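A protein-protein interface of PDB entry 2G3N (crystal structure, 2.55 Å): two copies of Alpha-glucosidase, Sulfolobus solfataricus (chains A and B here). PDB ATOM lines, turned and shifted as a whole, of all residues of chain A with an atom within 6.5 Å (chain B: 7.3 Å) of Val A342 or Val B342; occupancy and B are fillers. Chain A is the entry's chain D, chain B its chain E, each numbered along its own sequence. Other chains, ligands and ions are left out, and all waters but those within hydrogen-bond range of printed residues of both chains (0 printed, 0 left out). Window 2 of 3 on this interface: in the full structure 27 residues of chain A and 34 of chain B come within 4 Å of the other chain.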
ATOM      1  N   LEU A 337     -16.739  11.862 -10.089  1.00  0.00           N
ATOM      2  CA  LEU A 337     -15.793  10.844  -9.640  1.00  0.00           C
ATOM      3  C   LEU A 337     -16.367   9.428  -9.557  1.00  0.00           C
ATOM      4  O   LEU A 337     -15.783   8.556  -8.922  1.00  0.00           O
ATOM      5  CB  LEU A 337     -15.220  11.245  -8.278  1.00  0.00           C
ATOM      6  CG  LEU A 337     -14.647  12.661  -8.191  1.00  0.00           C
ATOM      7  CD1 LEU A 337     -14.220  12.941  -6.759  1.00  0.00           C
ATOM      8  CD2 LEU A 337     -13.473  12.817  -9.150  1.00  0.00           C
ATOM      9  N   SER A 339     -16.516   7.005 -11.753  1.00  0.00           N
ATOM     10  CA  SER A 339     -15.599   6.040 -12.355  1.00  0.00           C
ATOM     11  C   SER A 339     -14.494   5.583 -11.408  1.00  0.00           C
ATOM     12  O   SER A 339     -14.294   4.388 -11.194  1.00  0.00           O
ATOM     13  CB  SER A 339     -14.967   6.656 -13.606  1.00  0.00           C
ATOM     14  OG  SER A 339     -14.356   7.907 -13.311  1.00  0.00           O
ATOM     15  N   LEU A 340     -13.777   6.558 -10.866  1.00  0.00           N
ATOM     16  CA  LEU A 340     -12.675   6.338  -9.942  1.00  0.00           C
ATOM     17  C   LEU A 340     -13.020   5.262  -8.899  1.00  0.00           C
ATOM     18  O   LEU A 340     -14.065   5.328  -8.253  1.00  0.00           O
ATOM     19  CB  LEU A 340     -12.350   7.671  -9.268  1.00  0.00           C
ATOM     20  CG  LEU A 340     -11.035   7.872  -8.529  1.00  0.00           C
ATOM     21  CD1 LEU A 340      -9.862   7.609  -9.460  1.00  0.00           C
ATOM     22  CD2 LEU A 340     -10.996   9.297  -8.003  1.00  0.00           C
ATOM     23  N   PRO A 341     -12.142   4.255  -8.731  1.00  0.00           N
ATOM     24  CA  PRO A 341     -12.327   3.149  -7.779  1.00  0.00           C
ATOM     25  C   PRO A 341     -11.976   3.489  -6.326  1.00  0.00           C
ATOM     26  O   PRO A 341     -11.601   2.610  -5.547  1.00  0.00           O
ATOM     27  CB  PRO A 341     -11.412   2.069  -8.342  1.00  0.00           C
ATOM     28  CG  PRO A 341     -10.254   2.874  -8.841  1.00  0.00           C
ATOM     29  CD  PRO A 341     -10.935   4.034  -9.553  1.00  0.00           C
ATOM     30  N   VAL A 342     -12.116   4.758  -5.967  1.00  0.00           N
ATOM     31  CA  VAL A 342     -11.791   5.226  -4.624  1.00  0.00           C
ATOM     32  C   VAL A 342     -13.006   5.436  -3.721  1.00  0.00           C
ATOM     33  O   VAL A 342     -14.103   5.739  -4.194  1.00  0.00           O
ATOM     34  CB  VAL A 342     -10.991   6.538  -4.705  1.00  0.00           C
ATOM     35  CG1 VAL A 342     -10.782   7.115  -3.317  1.00  0.00           C
ATOM     36  CG2 VAL A 342      -9.652   6.278  -5.386  1.00  0.00           C
ATOM     37  N   GLN A 343     -12.792   5.274  -2.414  1.00  0.00           N
ATOM     38  CA  GLN A 343     -13.852   5.440  -1.425  1.00  0.00           C
ATOM     39  C   GLN A 343     -13.955   6.887  -0.948  1.00  0.00           C
ATOM     40  O   GLN A 343     -12.970   7.473  -0.502  1.00  0.00           O
ATOM     41  CB  GLN A 343     -13.600   4.531  -0.220  1.00  0.00           C
ATOM     42  CG  GLN A 343     -14.807   4.392   0.689  1.00  0.00           C
ATOM     43  CD  GLN A 343     -14.520   3.571   1.930  1.00  0.00           C
ATOM     44  OE1 GLN A 343     -13.937   2.487   1.854  1.00  0.00           O
ATOM     45  NE2 GLN A 343     -14.940   4.081   3.086  1.00  0.00           N
ATOM     46  N   PHE A 344     -15.155   7.452  -1.035  1.00  0.00           N
ATOM     47  CA  PHE A 344     -15.390   8.831  -0.622  1.00  0.00           C
ATOM     48  C   PHE A 344     -15.546   8.940   0.892  1.00  0.00           C
ATOM     49  O   PHE A 344     -15.863   7.964   1.566  1.00  0.00           O
ATOM     50  CB  PHE A 344     -16.660   9.375  -1.293  1.00  0.00           C
ATOM     51  CG  PHE A 344     -16.691   9.203  -2.792  1.00  0.00           C
ATOM     52  CD1 PHE A 344     -15.685   9.739  -3.595  1.00  0.00           C
ATOM     53  CD2 PHE A 344     -17.738   8.513  -3.402  1.00  0.00           C
ATOM     54  CE1 PHE A 344     -15.723   9.592  -4.986  1.00  0.00           C
ATOM     55  CE2 PHE A 344     -17.787   8.361  -4.790  1.00  0.00           C
ATOM     56  CZ  PHE A 344     -16.778   8.902  -5.581  1.00  0.00           C
ATOM     57  N   ARG A 345     -15.310  10.131   1.428  1.00  0.00           N
ATOM     58  CA  ARG A 345     -15.463  10.349   2.860  1.00  0.00           C
ATOM     59  C   ARG A 345     -16.916  10.770   3.035  1.00  0.00           C
ATOM     60  O   ARG A 345     -17.504  11.367   2.133  1.00  0.00           O
ATOM     61  CB  ARG A 345     -14.529  11.464   3.345  1.00  0.00           C
ATOM     62  CG  ARG A 345     -14.834  12.821   2.748  1.00  0.00           C
ATOM     63  CD  ARG A 345     -13.749  13.832   3.072  1.00  0.00           C
ATOM     64  NE  ARG A 345     -14.052  15.128   2.472  1.00  0.00           N
ATOM     65  CZ  ARG A 345     -13.197  16.142   2.403  1.00  0.00           C
ATOM     66  NH1 ARG A 345     -11.973  16.015   2.896  1.00  0.00           N
ATOM     67  NH2 ARG A 345     -13.568  17.284   1.836  1.00  0.00           N
ATOM     68  N   LEU B 337      -4.331  17.184  -1.187  1.00  0.00           N
ATOM     69  CA  LEU B 337      -5.588  16.513  -1.506  1.00  0.00           C
ATOM     70  C   LEU B 337      -6.731  16.879  -0.568  1.00  0.00           C
ATOM     71  O   LEU B 337      -7.749  16.194  -0.527  1.00  0.00           O
ATOM     72  CB  LEU B 337      -5.378  14.997  -1.489  1.00  0.00           C
ATOM     73  CG  LEU B 337      -4.205  14.487  -2.327  1.00  0.00           C
ATOM     74  CD1 LEU B 337      -4.039  12.996  -2.122  1.00  0.00           C
ATOM     75  CD2 LEU B 337      -4.440  14.799  -3.793  1.00  0.00           C
ATOM     76  N   SER B 338      -6.563  17.965   0.179  1.00  0.00           N
ATOM     77  CA  SER B 338      -7.574  18.420   1.134  1.00  0.00           C
ATOM     78  C   SER B 338      -8.958  18.634   0.536  1.00  0.00           C
ATOM     79  O   SER B 338      -9.975  18.413   1.196  1.00  0.00           O
ATOM     80  CB  SER B 338      -7.133  19.733   1.784  1.00  0.00           C
ATOM     81  OG  SER B 338      -6.869  20.726   0.802  1.00  0.00           O
ATOM     82  N   SER B 339      -8.987  19.082  -0.711  1.00  0.00           N
ATOM     83  CA  SER B 339     -10.235  19.364  -1.404  1.00  0.00           C
ATOM     84  C   SER B 339     -11.011  18.130  -1.841  1.00  0.00           C
ATOM     85  O   SER B 339     -12.239  18.131  -1.802  1.00  0.00           O
ATOM     86  CB  SER B 339      -9.941  20.209  -2.624  1.00  0.00           C
ATOM     87  OG  SER B 339      -9.007  19.535  -3.454  1.00  0.00           O
ATOM     88  N   LEU B 340     -10.305  17.089  -2.275  1.00  0.00           N
ATOM     89  CA  LEU B 340     -10.971  15.870  -2.717  1.00  0.00           C
ATOM     90  C   LEU B 340     -11.805  15.222  -1.620  1.00  0.00           C
ATOM     91  O   LEU B 340     -11.318  14.967  -0.517  1.00  0.00           O
ATOM     92  CB  LEU B 340      -9.962  14.857  -3.260  1.00  0.00           C
ATOM     93  CG  LEU B 340      -9.514  15.095  -4.701  1.00  0.00           C
ATOM     94  CD1 LEU B 340      -8.832  13.837  -5.224  1.00  0.00           C
ATOM     95  CD2 LEU B 340     -10.720  15.434  -5.571  1.00  0.00           C
ATOM     96  N   PRO B 341     -13.085  14.948  -1.920  1.00  0.00           N
ATOM     97  CA  PRO B 341     -14.029  14.330  -0.986  1.00  0.00           C
ATOM     98  C   PRO B 341     -13.774  12.836  -0.798  1.00  0.00           C
ATOM     99  O   PRO B 341     -14.687  12.079  -0.464  1.00  0.00           O
ATOM    100  CB  PRO B 341     -15.374  14.609  -1.640  1.00  0.00           C
ATOM    101  CG  PRO B 341     -15.042  14.470  -3.090  1.00  0.00           C
ATOM    102  CD  PRO B 341     -13.738  15.232  -3.210  1.00  0.00           C
ATOM    103  N   VAL B 342     -12.531  12.419  -1.015  1.00  0.00           N
ATOM    104  CA  VAL B 342     -12.158  11.017  -0.866  1.00  0.00           C
ATOM    105  C   VAL B 342     -11.686  10.726   0.558  1.00  0.00           C
ATOM    106  O   VAL B 342     -11.608  11.624   1.394  1.00  0.00           O
ATOM    107  CB  VAL B 342     -11.038  10.628  -1.865  1.00  0.00           C
ATOM    108  CG1 VAL B 342     -11.514  10.866  -3.296  1.00  0.00           C
ATOM    109  CG2 VAL B 342      -9.775  11.430  -1.578  1.00  0.00           C
ATOM    110  N   GLN B 343     -11.373   9.469   0.833  1.00  0.00           N
ATOM    111  CA  GLN B 343     -10.922   9.085   2.161  1.00  0.00           C
ATOM    112  C   GLN B 343      -9.485   8.592   2.098  1.00  0.00           C
ATOM    113  O   GLN B 343      -9.140   7.764   1.255  1.00  0.00           O
ATOM    114  CB  GLN B 343     -11.818   7.976   2.714  1.00  0.00           C
ATOM    115  CG  GLN B 343     -11.813   7.857   4.229  1.00  0.00           C
ATOM    116  CD  GLN B 343     -11.793   6.416   4.688  1.00  0.00           C
ATOM    117  OE1 GLN B 343     -12.469   5.560   4.111  1.00  0.00           O
ATOM    118  NE2 GLN B 343     -11.022   6.138   5.736  1.00  0.00           N
ATOM    119  N   PHE B 344      -8.647   9.100   2.993  1.00  0.00           N
ATOM    120  CA  PHE B 344      -7.247   8.703   3.023  1.00  0.00           C
ATOM    121  C   PHE B 344      -7.073   7.422   3.817  1.00  0.00           C
ATOM    122  O   PHE B 344      -7.651   7.264   4.890  1.00  0.00           O
ATOM    123  CB  PHE B 344      -6.399   9.796   3.665  1.00  0.00           C
ATOM    124  CG  PHE B 344      -6.592  11.146   3.056  1.00  0.00           C
ATOM    125  CD1 PHE B 344      -6.227  11.384   1.738  1.00  0.00           C
ATOM    126  CD2 PHE B 344      -7.144  12.182   3.800  1.00  0.00           C
ATOM    127  CE1 PHE B 344      -6.407  12.637   1.170  1.00  0.00           C
ATOM    128  CE2 PHE B 344      -7.329  13.436   3.246  1.00  0.00           C
ATOM    129  CZ  PHE B 344      -6.960  13.667   1.927  1.00  0.00           C
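The backbone NH of Arg A345 lies within hydrogen-bond range of the backbone carbonyl oxygen of Pro B341 (2.8 Å). The backbone NH of Gln B343 lies within hydrogen-bond range of the backbone carbonyl oxygen of Gln A343 (2.9 Å).
Among the printed residues, pairs that only touch across the chains: Val A342 with Val B342 (3.8 Å), Gln A343 with Val B342 (3.7 Å), Phe A344 with Pro B341 (3.3 Å), Phe A344 with Val B342 (3.9 Å), Arg A345 with Ser B338 (3.6 Å), Arg A345 with Ser B339 (3.96 Å), Arg A345 with Leu B340 (3.6 Å) and Arg A345 with Val B342 (3.5 Å).
Of chain A, only Val A342 (3.8 Å), Gln A343 (3.7 Å), Phe A344 (3.9 Å) and Arg A345 (3.5 Å) come within 4 Å of Val B342. Printed residues of chain A within 4 Å of Leu B340: Arg A345. Of the printed residues of chain A, Ser B339 touches Arg A345 (3.96 Å). Of the printed residues of chain A, Ser B338 touches Arg A345 (3.6 Å). Printed residues of chain B within 4 Å of Phe A344: Pro B341 and Val B342. Printed residues of chain B within 4 Å of Gln A343: Val B342 (3.7 Å) and Gln B343 (2.9 Å). Pro A341 touches none of the printed residues of chain B. Ser A339 touches none of the printed residues of chain B. The nearest residue of chain A that does not touch Val B342 is Leu A337 (4.9 Å).
Of the 8 printed residues of chain B, 6 touch a printed residue of chain A. Hydrophobic or aromatic side chains of chain B within 4 Å of the printed part of chain A: Val B342. Of the 8 printed residues of chain A, 4 touch a printed residue of chain B. Hydrophobic or aromatic side chains of chain A within 4 Å of the printed part of chain B: Val A342 and Phe A344. Among the printed residues, no Asp or Glu carboxylate lies within 4 Å of a Lys or Arg side-chain nitrogen of the other chain.
Val B342 touches its own counterpart, Val A342. Gln B343 touches its own counterpart, Gln A343. Phe A344 touches Pro B341, but with the chains exchanged Pro A341 does not touch Phe B344 (11.1 Å). Phe A344 touches Val B342, but with the chains exchanged Val A342 does not touch Phe B344 (7.0 Å). Of the 10 pairs that touch across the chains among the printed residues, 2 have their exchanged pair printed and touching as well.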
